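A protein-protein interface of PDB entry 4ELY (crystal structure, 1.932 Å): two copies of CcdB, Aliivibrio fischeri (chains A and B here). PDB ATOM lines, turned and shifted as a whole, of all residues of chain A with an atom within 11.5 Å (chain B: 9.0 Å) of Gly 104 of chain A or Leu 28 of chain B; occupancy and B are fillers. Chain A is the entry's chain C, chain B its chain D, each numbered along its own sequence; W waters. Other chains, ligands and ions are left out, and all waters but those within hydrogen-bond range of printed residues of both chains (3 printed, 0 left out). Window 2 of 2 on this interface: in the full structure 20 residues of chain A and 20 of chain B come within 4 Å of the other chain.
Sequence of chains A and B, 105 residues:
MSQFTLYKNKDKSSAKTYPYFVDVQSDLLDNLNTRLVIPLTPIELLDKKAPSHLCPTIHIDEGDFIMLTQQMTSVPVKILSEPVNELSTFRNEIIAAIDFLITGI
Among the printed residues, pairs that only touch across the chains: Ile 102 of chain A with Ile 95 of chain B, Ile 102 of chain A with Val 24 of chain B, Leu 101 of chain A with Gln 25 of chain B, Leu 101 of chain A with Leu 29 of chain B, Gly 104 of chain A with Ser 26 of chain B, Phe 100 of chain A with Leu 29 of chain B, Gly 104 of chain A with Leu 28 of chain B, Leu 54 of chain A with Leu 32 of chain B, Gln 70 of chain A with Leu 32 of chain B, Phe 100 of chain A with Ser 26 of chain B and Ile 102 of chain A with Ser 26 of chain B.
Water W1 lies within hydrogen-bond range of OE1 of Gln 25 of chain B (2.6 Å), O of Gln 70 of chain A (3.0 Å) and N of Arg 35 of chain B (3.4 Å). Water W2 lies within hydrogen-bond range of OG of Ser 26 of chain B (2.7 Å) and O of Thr 103 of chain A (3.5 Å). Water W3 lies within hydrogen-bond range of the backbone carbonyl oxygen of Thr 103 of chain A and the guanidinium group of Arg 91 of chain B.
O of Leu 29 of chain B is in hydrogen-bond range of NE2 of Gln 25 of chain B (3.5 Å). O of Leu 54 of chain A lies within hydrogen-bond range of OG1 of Thr 69 of chain A (2.6 Å). The guanidinium group (NH1) of Arg 35 of chain B sits at hydrogen-bond distance from the backbone carbonyl oxygen (O) of Leu 32 of chain B (2.7 Å). The backbone NH of Gln 3 of chain B lies within hydrogen-bond range of the side-chain carboxylate of Asp 27 of chain B. The backbone carbonyl oxygen of Asp 99 of chain A is in hydrogen-bond range of the backbone NH of Gly 104 of chain A. The side-chain amide nitrogen (NE2) of Gln 3 of chain B lies within hydrogen-bond range of the backbone carbonyl oxygen (O) of Val 24 of chain B (3.0 Å).
NE2 of Gln 3 of chain B is in hydrogen-bond range of O of Ile 102 of chain A (2.7 Å). The backbone carbonyl oxygen (O) of Leu 101 of chain A lies within hydrogen-bond range of the backbone NH (N) of Ser 26 of chain B (2.8 Å).
Gly 104 of chain A touches just these residues of chain B: Ser 26 and Leu 28. No residue of chain B comes within 4 Å of Thr 103 of chain A. No residue of chain B comes within 4 Å of Ile 105 of chain A. Ser 26 of chain B touches just these residues of chain A: Phe 100 (3.8 Å), Leu 101 (2.8 Å), Ile 102 (3.9 Å) and Gly 104 (3.7 Å). No residue of chain A comes within 4 Å of Asp 27 of chain B. Of the printed residues of chain B, Phe 100 of chain A touches Ser 26 (3.8 Å) and Leu 29 (3.7 Å). Of the printed residues of chain A, Ile 95 of chain B touches Ile 102. Of the printed residues of chain A, Val 24 of chain B touches Ile 102. Printed residues of chain A within 4 Å of Gln 25 of chain B: Leu 101. Thr 69 of chain A touches none of the printed residues of chain B. The nearest residue of chain B that does not touch Gly 104 of chain A is Gln 3 of chain B (6.1 Å). The nearest residue of chain A that does not touch Leu 28 of chain B is Phe 100 of chain A (4.7 Å).
1 position is printed for both chains. Of the 13 pairs that touch across the chains among the printed residues, none has its exchanged pair printed and touching as well.
Printed residues of chain B that touch a printed residue of chain A: Gln 3, Val 24, Gln 25, Ser 26, Leu 28, Leu 29, Leu 32 and Ile 95. Along chain B the printed residues that touch a printed residue of chain A span positions 3 to 95. Hydrophobic or aromatic side chains of chain A within 4 Å of the printed part of chain B: Leu 54, Phe 100, Leu 101 and Ile 102. Among the printed residues, 13 pairs touch across the chains. Among the printed residues, no Asp or Glu carboxylate lies within 4 Å of a Lys or Arg side-chain nitrogen of the other chain.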
ATOM      1  N   PRO A  51     -24.550 -36.852   4.560  1.00  0.00           N
ATOM      2  CA  PRO A  51     -24.387 -35.414   4.331  1.00  0.00           C
ATOM      3  C   PRO A  51     -25.746 -34.708   4.399  1.00  0.00           C
ATOM      4  O   PRO A  51     -26.415 -34.548   3.376  1.00  0.00           O
ATOM      5  CB  PRO A  51     -23.805 -35.354   2.908  1.00  0.00           C
ATOM      6  CG  PRO A  51     -23.939 -36.788   2.334  1.00  0.00           C
ATOM      7  CD  PRO A  51     -24.777 -37.572   3.297  1.00  0.00           C
ATOM      8  N   HIS A  53     -27.120 -31.608   4.842  1.00  0.00           N
ATOM      9  CA  HIS A  53     -27.462 -30.414   4.072  1.00  0.00           C
ATOM     10  C   HIS A  53     -27.724 -30.774   2.599  1.00  0.00           C
ATOM     11  O   HIS A  53     -28.626 -30.226   1.953  1.00  0.00           O
ATOM     12  CB  HIS A  53     -26.318 -29.394   4.214  1.00  0.00           C
ATOM     13  CG  HIS A  53     -26.621 -28.038   3.654  1.00  0.00           C
ATOM     14  ND1 HIS A  53     -27.883 -27.483   3.669  1.00  0.00           N
ATOM     15  CD2 HIS A  53     -25.813 -27.115   3.068  1.00  0.00           C
ATOM     16  CE1 HIS A  53     -27.842 -26.282   3.115  1.00  0.00           C
ATOM     17  NE2 HIS A  53     -26.599 -26.037   2.743  1.00  0.00           N
ATOM     18  N   LEU A  54     -26.945 -31.712   2.073  1.00  0.00           N
ATOM     19  CA  LEU A  54     -27.127 -32.168   0.686  1.00  0.00           C
ATOM     20  C   LEU A  54     -28.306 -33.138   0.495  1.00  0.00           C
ATOM     21  O   LEU A  54     -28.974 -33.128  -0.544  1.00  0.00           O
ATOM     22  CB  LEU A  54     -25.846 -32.835   0.202  1.00  0.00           C
ATOM     23  CG  LEU A  54     -25.854 -33.272  -1.262  1.00  0.00           C
ATOM     24  CD1 LEU A  54     -26.055 -32.045  -2.136  1.00  0.00           C
ATOM     25  CD2 LEU A  54     -24.558 -33.973  -1.606  1.00  0.00           C
ATOM     26  N   THR A  69     -30.127 -35.780  -3.642  1.00  0.00           N
ATOM     27  CA  THR A  69     -30.057 -34.578  -4.472  1.00  0.00           C
ATOM     28  C   THR A  69     -28.953 -34.670  -5.526  1.00  0.00           C
ATOM     29  O   THR A  69     -29.130 -34.242  -6.670  1.00  0.00           O
ATOM     30  CB  THR A  69     -29.795 -33.354  -3.578  1.00  0.00           C
ATOM     31  OG1 THR A  69     -30.740 -33.344  -2.492  1.00  0.00           O
ATOM     32  CG2 THR A  69     -29.903 -32.053  -4.371  1.00  0.00           C
ATOM     33  N   GLN A  70     -27.815 -35.241  -5.149  1.00  0.00           N
ATOM     34  CA  GLN A  70     -26.702 -35.350  -6.084  1.00  0.00           C
ATOM     35  C   GLN A  70     -27.014 -36.304  -7.231  1.00  0.00           C
ATOM     36  O   GLN A  70     -26.373 -36.233  -8.273  1.00  0.00           O
ATOM     37  CB  GLN A  70     -25.418 -35.797  -5.370  1.00  0.00           C
ATOM     38  CG  GLN A  70     -25.395 -37.274  -4.954  1.00  0.00           C
ATOM     39  CD  GLN A  70     -26.009 -37.512  -3.588  1.00  0.00           C
ATOM     40  OE1 GLN A  70     -26.937 -36.816  -3.179  1.00  0.00           O
ATOM     41  NE2 GLN A  70     -25.481 -38.497  -2.868  1.00  0.00           N
ATOM     42  N   ILE A  94     -35.484 -28.800   0.035  1.00  0.00           N
ATOM     43  CA  ILE A  94     -35.146 -29.229  -1.323  1.00  0.00           C
ATOM     44  C   ILE A  94     -34.346 -28.174  -2.080  1.00  0.00           C
ATOM     45  O   ILE A  94     -33.291 -28.471  -2.672  1.00  0.00           O
ATOM     46  CB  ILE A  94     -36.420 -29.647  -2.107  1.00  0.00           C
ATOM     47  CG1 ILE A  94     -37.001 -30.921  -1.483  1.00  0.00           C
ATOM     48  CG2 ILE A  94     -36.093 -29.851  -3.581  1.00  0.00           C
ATOM     49  CD1 ILE A  94     -38.394 -31.319  -1.998  1.00  0.00           C
ATOM     50  N   ILE A  95     -34.826 -26.931  -2.050  1.00  0.00           N
ATOM     51  CA  ILE A  95     -34.109 -25.838  -2.704  1.00  0.00           C
ATOM     52  C   ILE A  95     -32.723 -25.597  -2.088  1.00  0.00           C
ATOM     53  O   ILE A  95     -31.741 -25.380  -2.813  1.00  0.00           O
ATOM     54  CB  ILE A  95     -34.911 -24.519  -2.656  1.00  0.00           C
ATOM     55  CG1 ILE A  95     -36.270 -24.697  -3.350  1.00  0.00           C
ATOM     56  CG2 ILE A  95     -34.099 -23.367  -3.279  1.00  0.00           C
ATOM     57  CD1 ILE A  95     -36.189 -25.205  -4.776  1.00  0.00           C
ATOM     58  N   ALA A  96     -32.650 -25.624  -0.758  1.00  0.00           N
ATOM     59  CA  ALA A  96     -31.368 -25.505  -0.057  1.00  0.00           C
ATOM     60  C   ALA A  96     -30.369 -26.571  -0.497  1.00  0.00           C
ATOM     61  O   ALA A  96     -29.201 -26.263  -0.685  1.00  0.00           O
ATOM     62  CB  ALA A  96     -31.566 -25.552   1.466  1.00  0.00           C
ATOM     63  N   ALA A  97     -30.824 -27.816  -0.652  1.00  0.00           N
ATOM     64  CA  ALA A  97     -29.946 -28.912  -1.083  1.00  0.00           C
ATOM     65  C   ALA A  97     -29.430 -28.688  -2.494  1.00  0.00           C
ATOM     66  O   ALA A  97     -28.251 -28.902  -2.776  1.00  0.00           O
ATOM     67  CB  ALA A  97     -30.674 -30.243  -1.023  1.00  0.00           C
ATOM     68  N   ILE A  98     -30.319 -28.288  -3.397  1.00  0.00           N
ATOM     69  CA  ILE A  98     -29.900 -28.015  -4.770  1.00  0.00           C
ATOM     70  C   ILE A  98     -28.926 -26.833  -4.800  1.00  0.00           C
ATOM     71  O   ILE A  98     -27.935 -26.848  -5.542  1.00  0.00           O
ATOM     72  CB  ILE A  98     -31.119 -27.735  -5.675  1.00  0.00           C
ATOM     73  CG1 ILE A  98     -31.995 -28.987  -5.762  1.00  0.00           C
ATOM     74  CG2 ILE A  98     -30.667 -27.274  -7.065  1.00  0.00           C
ATOM     75  CD1 ILE A  98     -33.369 -28.748  -6.384  1.00  0.00           C
ATOM     76  N   ASP A  99     -29.201 -25.802  -4.000  1.00  0.00           N
ATOM     77  CA  ASP A  99     -28.299 -24.647  -3.940  1.00  0.00           C
ATOM     78  C   ASP A  99     -26.926 -25.042  -3.428  1.00  0.00           C
ATOM     79  O   ASP A  99     -25.911 -24.506  -3.858  1.00  0.00           O
ATOM     80  CB  ASP A  99     -28.857 -23.542  -3.032  1.00  0.00           C
ATOM     81  CG  ASP A  99     -29.927 -22.701  -3.708  1.00  0.00           C
ATOM     82  OD1 ASP A  99     -30.062 -22.782  -4.949  1.00  0.00           O
ATOM     83  OD2 ASP A  99     -30.632 -21.949  -2.996  1.00  0.00           O
ATOM     84  N   PHE A 100     -26.900 -25.967  -2.482  1.00  0.00           N
ATOM     85  CA  PHE A 100     -25.625 -26.437  -1.942  1.00  0.00           C
ATOM     86  C   PHE A 100     -24.865 -27.195  -3.023  1.00  0.00           C
ATOM     87  O   PHE A 100     -23.654 -27.019  -3.202  1.00  0.00           O
ATOM     88  CB  PHE A 100     -25.907 -27.354  -0.750  1.00  0.00           C
ATOM     89  CG  PHE A 100     -24.674 -27.882  -0.082  1.00  0.00           C
ATOM     90  CD1 PHE A 100     -23.572 -27.058   0.130  1.00  0.00           C
ATOM     91  CD2 PHE A 100     -24.615 -29.200   0.339  1.00  0.00           C
ATOM     92  CE1 PHE A 100     -22.430 -27.540   0.749  1.00  0.00           C
ATOM     93  CE2 PHE A 100     -23.472 -29.694   0.972  1.00  0.00           C
ATOM     94  CZ  PHE A 100     -22.382 -28.865   1.180  1.00  0.00           C
ATOM     95  N   LEU A 101     -25.578 -28.045  -3.750  1.00  0.00           N
ATOM     96  CA  LEU A 101     -24.947 -28.855  -4.798  1.00  0.00           C
ATOM     97  C   LEU A 101     -24.317 -28.000  -5.904  1.00  0.00           C
ATOM     98  O   LEU A 101     -23.253 -28.327  -6.440  1.00  0.00           O
ATOM     99  CB  LEU A 101     -25.982 -29.820  -5.394  1.00  0.00           C
ATOM    100  CG  LEU A 101     -25.472 -30.804  -6.450  1.00  0.00           C
ATOM    101  CD1 LEU A 101     -24.566 -31.817  -5.789  1.00  0.00           C
ATOM    102  CD2 LEU A 101     -26.640 -31.500  -7.153  1.00  0.00           C
ATOM    103  N   ILE A 102     -24.968 -26.886  -6.226  1.00  0.00           N
ATOM    104  CA  ILE A 102     -24.546 -26.049  -7.351  1.00  0.00           C
ATOM    105  C   ILE A 102     -23.756 -24.817  -6.921  1.00  0.00           C
ATOM    106  O   ILE A 102     -22.709 -24.512  -7.486  1.00  0.00           O
ATOM    107  CB  ILE A 102     -25.747 -25.539  -8.164  1.00  0.00           C
ATOM    108  CG1 ILE A 102     -26.611 -26.705  -8.640  1.00  0.00           C
ATOM    109  CG2 ILE A 102     -25.239 -24.759  -9.344  1.00  0.00           C
ATOM    110  CD1 ILE A 102     -25.842 -27.682  -9.405  1.00  0.00           C
ATOM    111  N   THR A 103     -24.268 -24.094  -5.930  1.00  0.00           N
ATOM    112  CA  THR A 103     -23.618 -22.844  -5.541  1.00  0.00           C
ATOM    113  C   THR A 103     -22.750 -22.991  -4.302  1.00  0.00           C
ATOM    114  O   THR A 103     -22.043 -22.061  -3.926  1.00  0.00           O
ATOM    115  CB  THR A 103     -24.625 -21.673  -5.378  1.00  0.00           C
ATOM    116  OG1 THR A 103     -25.678 -22.054  -4.493  1.00  0.00           O
ATOM    117  CG2 THR A 103     -25.210 -21.294  -6.716  1.00  0.00           C
ATOM    118  N   GLY A 104     -22.808 -24.157  -3.668  1.00  0.00           N
ATOM    119  CA  GLY A 104     -22.019 -24.387  -2.474  1.00  0.00           C
ATOM    120  C   GLY A 104     -22.540 -23.605  -1.271  1.00  0.00           C
ATOM    121  O   GLY A 104     -21.812 -23.405  -0.299  1.00  0.00           O
ATOM    122  N   ILE A 105     -23.795 -23.164  -1.325  1.00  0.00           N
ATOM    123  CA  ILE A 105     -24.355 -22.404  -0.200  1.00  0.00           C
ATOM    124  C   ILE A 105     -24.846 -23.343   0.910  1.00  0.00           C
ATOM    125  O   ILE A 105     -25.618 -24.266   0.651  1.00  0.00           O
ATOM    126  CB  ILE A 105     -25.515 -21.490  -0.634  1.00  0.00           C
ATOM    127  CG1 ILE A 105     -25.028 -20.414  -1.616  1.00  0.00           C
ATOM    128  CG2 ILE A 105     -26.192 -20.865   0.609  1.00  0.00           C
ATOM    129  CD1 ILE A 105     -24.023 -19.460  -1.061  1.00  0.00           C
ATOM    130  OXT ILE A 105     -24.507 -23.204   2.097  1.00  0.00           O
ATOM    131  N   SER B   2     -14.502 -30.939 -12.246  1.00  0.00           N
ATOM    132  CA  SER B   2     -14.182 -29.617 -11.682  1.00  0.00           C
ATOM    133  C   SER B   2     -15.207 -28.577 -12.151  1.00  0.00           C
ATOM    134  O   SER B   2     -15.554 -28.558 -13.330  1.00  0.00           O
ATOM    135  CB  SER B   2     -12.771 -29.209 -12.102  1.00  0.00           C
ATOM    136  OG  SER B   2     -12.409 -27.963 -11.534  1.00  0.00           O
ATOM    137  N   GLN B   3     -15.702 -27.720 -11.252  1.00  0.00           N
ATOM    138  CA  GLN B   3     -16.858 -26.881 -11.606  1.00  0.00           C
ATOM    139  C   GLN B   3     -16.603 -25.984 -12.825  1.00  0.00           C
ATOM    140  O   GLN B   3     -15.630 -25.221 -12.866  1.00  0.00           O
ATOM    141  CB  GLN B   3     -17.399 -26.044 -10.431  1.00  0.00           C
ATOM    142  CG  GLN B   3     -18.864 -25.638 -10.686  1.00  0.00           C
ATOM    143  CD  GLN B   3     -19.488 -24.819  -9.565  1.00  0.00           C
ATOM    144  OE1 GLN B   3     -18.810 -24.044  -8.890  1.00  0.00           O
ATOM    145  NE2 GLN B   3     -20.788 -24.981  -9.380  1.00  0.00           N
ATOM    146  N   VAL B  24     -21.329 -28.938 -13.395  1.00  0.00           N
ATOM    147  CA  VAL B  24     -21.893 -27.754 -12.738  1.00  0.00           C
ATOM    148  C   VAL B  24     -21.954 -27.924 -11.232  1.00  0.00           C
ATOM    149  O   VAL B  24     -22.578 -27.133 -10.529  1.00  0.00           O
ATOM    150  CB  VAL B  24     -23.301 -27.400 -13.273  1.00  0.00           C
ATOM    151  CG1 VAL B  24     -23.209 -27.058 -14.768  1.00  0.00           C
ATOM    152  CG2 VAL B  24     -24.278 -28.556 -13.019  1.00  0.00           C
ATOM    153  N   GLN B  25     -21.279 -28.954 -10.739  1.00  0.00           N
ATOM    154  CA  GLN B  25     -21.324 -29.276  -9.322  1.00  0.00           C
ATOM    155  C   GLN B  25     -20.262 -28.494  -8.557  1.00  0.00           C
ATOM    156  O   GLN B  25     -19.129 -28.349  -9.018  1.00  0.00           O
ATOM    157  CB  GLN B  25     -21.107 -30.771  -9.133  1.00  0.00           C
ATOM    158  CG  GLN B  25     -21.300 -31.275  -7.725  1.00  0.00           C
ATOM    159  CD  GLN B  25     -21.437 -32.784  -7.697  1.00  0.00           C
ATOM    160  OE1 GLN B  25     -22.438 -33.338  -8.162  1.00  0.00           O
ATOM    161  NE2 GLN B  25     -20.426 -33.460  -7.159  1.00  0.00           N
ATOM    162  N   SER B  26     -20.631 -27.999  -7.381  1.00  0.00           N
ATOM    163  CA  SER B  26     -19.710 -27.245  -6.536  1.00  0.00           C
ATOM    164  C   SER B  26     -18.497 -28.083  -6.130  1.00  0.00           C
ATOM    165  O   SER B  26     -18.639 -29.261  -5.785  1.00  0.00           O
ATOM    166  CB  SER B  26     -20.428 -26.770  -5.270  1.00  0.00           C
ATOM    167  OG  SER B  26     -19.486 -26.276  -4.328  1.00  0.00           O
ATOM    168  N   ASP B  27     -17.319 -27.471  -6.139  1.00  0.00           N
ATOM    169  CA  ASP B  27     -16.088 -28.200  -5.839  1.00  0.00           C
ATOM    170  C   ASP B  27     -16.036 -28.621  -4.365  1.00  0.00           C
ATOM    171  O   ASP B  27     -15.236 -29.479  -3.997  1.00  0.00           O
ATOM    172  CB  ASP B  27     -14.851 -27.365  -6.195  1.00  0.00           C
ATOM    173  CG  ASP B  27     -14.706 -27.128  -7.695  1.00  0.00           C
ATOM    174  OD1 ASP B  27     -15.186 -27.960  -8.495  1.00  0.00           O
ATOM    175  OD2 ASP B  27     -14.105 -26.100  -8.072  1.00  0.00           O
ATOM    176  N   LEU B  28     -16.884 -28.017  -3.529  1.00  0.00           N
ATOM    177  CA  LEU B  28     -16.999 -28.419  -2.122  1.00  0.00           C
ATOM    178  C   LEU B  28     -17.532 -29.855  -1.986  1.00  0.00           C
ATOM    179  O   LEU B  28     -17.430 -30.472  -0.928  1.00  0.00           O
ATOM    180  CB  LEU B  28     -17.914 -27.454  -1.342  1.00  0.00           C
ATOM    181  CG  LEU B  28     -17.450 -26.002  -1.162  1.00  0.00           C
ATOM    182  CD1 LEU B  28     -18.559 -25.137  -0.563  1.00  0.00           C
ATOM    183  CD2 LEU B  28     -16.205 -25.929  -0.294  1.00  0.00           C
ATOM    184  N   LEU B  29     -18.101 -30.386  -3.061  1.00  0.00           N
ATOM    185  CA  LEU B  29     -18.658 -31.733  -3.025  1.00  0.00           C
ATOM    186  C   LEU B  29     -17.870 -32.716  -3.889  1.00  0.00           C
ATOM    187  O   LEU B  29     -18.411 -33.732  -4.330  1.00  0.00           O
ATOM    188  CB  LEU B  29     -20.119 -31.691  -3.464  1.00  0.00           C
ATOM    189  CG  LEU B  29     -20.987 -30.859  -2.518  1.00  0.00           C
ATOM    190  CD1 LEU B  29     -22.331 -30.583  -3.133  1.00  0.00           C
ATOM    191  CD2 LEU B  29     -21.157 -31.580  -1.187  1.00  0.00           C
ATOM    192  N   ASP B  30     -16.591 -32.437  -4.127  1.00  0.00           N
ATOM    193  CA  ASP B  30     -15.828 -33.302  -5.035  1.00  0.00           C
ATOM    194  C   ASP B  30     -15.464 -34.654  -4.409  1.00  0.00           C
ATOM    195  O   ASP B  30     -14.943 -35.540  -5.082  1.00  0.00           O
ATOM    196  CB  ASP B  30     -14.609 -32.588  -5.648  1.00  0.00           C
ATOM    197  CG  ASP B  30     -13.632 -32.074  -4.607  1.00  0.00           C
ATOM    198  OD1 ASP B  30     -13.491 -32.705  -3.537  1.00  0.00           O
ATOM    199  OD2 ASP B  30     -12.984 -31.036  -4.871  1.00  0.00           O
ATOM    200  N   ASN B  31     -15.755 -34.809  -3.122  1.00  0.00           N
ATOM    201  CA  ASN B  31     -15.587 -36.101  -2.463  1.00  0.00           C
ATOM    202  C   ASN B  31     -16.604 -37.135  -2.966  1.00  0.00           C
ATOM    203  O   ASN B  31     -16.351 -38.341  -2.926  1.00  0.00           O
ATOM    204  CB  ASN B  31     -15.663 -35.939  -0.943  1.00  0.00           C
ATOM    205  CG  ASN B  31     -16.771 -34.989  -0.508  1.00  0.00           C
ATOM    206  OD1 ASN B  31     -16.673 -33.768  -0.694  1.00  0.00           O
ATOM    207  ND2 ASN B  31     -17.828 -35.543   0.087  1.00  0.00           N
ATOM    208  N   LEU B  32     -17.745 -36.649  -3.454  1.00  0.00           N
ATOM    209  CA  LEU B  32     -18.767 -37.504  -4.059  1.00  0.00           C
ATOM    210  C   LEU B  32     -18.217 -38.230  -5.284  1.00  0.00           C
ATOM    211  O   LEU B  32     -17.387 -37.686  -6.017  1.00  0.00           O
ATOM    212  CB  LEU B  32     -19.979 -36.665  -4.474  1.00  0.00           C
ATOM    213  CG  LEU B  32     -20.743 -35.955  -3.355  1.00  0.00           C
ATOM    214  CD1 LEU B  32     -21.929 -35.215  -3.941  1.00  0.00           C
ATOM    215  CD2 LEU B  32     -21.201 -36.960  -2.305  1.00  0.00           C
ATOM    216  N   ARG B  35     -20.941 -36.547 -10.388  1.00  0.00           N
ATOM    217  CA  ARG B  35     -20.958 -35.130 -10.715  1.00  0.00           C
ATOM    218  C   ARG B  35     -22.247 -34.796 -11.440  1.00  0.00           C
ATOM    219  O   ARG B  35     -22.681 -35.533 -12.329  1.00  0.00           O
ATOM    220  CB  ARG B  35     -19.773 -34.764 -11.610  1.00  0.00           C
ATOM    221  CG  ARG B  35     -18.409 -34.978 -10.983  1.00  0.00           C
ATOM    222  CD  ARG B  35     -18.105 -33.932  -9.903  1.00  0.00           C
ATOM    223  NE  ARG B  35     -16.752 -34.114  -9.361  1.00  0.00           N
ATOM    224  CZ  ARG B  35     -16.477 -34.857  -8.292  1.00  0.00           C
ATOM    225  NH1 ARG B  35     -17.456 -35.473  -7.635  1.00  0.00           N
ATOM    226  NH2 ARG B  35     -15.231 -34.972  -7.866  1.00  0.00           N
ATOM    227  N   ARG B  91     -20.515 -18.665 -16.031  1.00  0.00           N
ATOM    228  CA  ARG B  91     -21.085 -19.057 -14.733  1.00  0.00           C
ATOM    229  C   ARG B  91     -22.449 -18.442 -14.485  1.00  0.00           C
ATOM    230  O   ARG B  91     -23.376 -19.120 -14.073  1.00  0.00           O
ATOM    231  CB  ARG B  91     -20.160 -18.636 -13.582  1.00  0.00           C
ATOM    232  CG  ARG B  91     -20.706 -19.033 -12.221  1.00  0.00           C
ATOM    233  CD  ARG B  91     -19.924 -18.425 -11.063  1.00  0.00           C
ATOM    234  NE  ARG B  91     -20.185 -19.192  -9.843  1.00  0.00           N
ATOM    235  CZ  ARG B  91     -21.245 -19.020  -9.055  1.00  0.00           C
ATOM    236  NH1 ARG B  91     -22.158 -18.098  -9.344  1.00  0.00           N
ATOM    237  NH2 ARG B  91     -21.393 -19.774  -7.970  1.00  0.00           N
ATOM    238  N   ILE B  95     -25.904 -20.660 -14.000  1.00  0.00           N
ATOM    239  CA  ILE B  95     -26.656 -20.681 -12.743  1.00  0.00           C
ATOM    240  C   ILE B  95     -28.060 -20.112 -12.945  1.00  0.00           C
ATOM    241  O   ILE B  95     -29.036 -20.634 -12.412  1.00  0.00           O
ATOM    242  CB  ILE B  95     -25.956 -19.862 -11.631  1.00  0.00           C
ATOM    243  CG1 ILE B  95     -24.538 -20.384 -11.373  1.00  0.00           C
ATOM    244  CG2 ILE B  95     -26.793 -19.850 -10.348  1.00  0.00           C
ATOM    245  CD1 ILE B  95     -24.477 -21.822 -10.989  1.00  0.00           C
HETATM  246  O   HOH W   1     -23.469 -35.685  -8.211  1.00  0.00           O
HETATM  247  O   HOH W   2     -19.105 -23.619  -4.851  1.00  0.00           O
HETATM  248  O   HOH W   3     -21.306 -19.464  -4.832  1.00  0.00           O
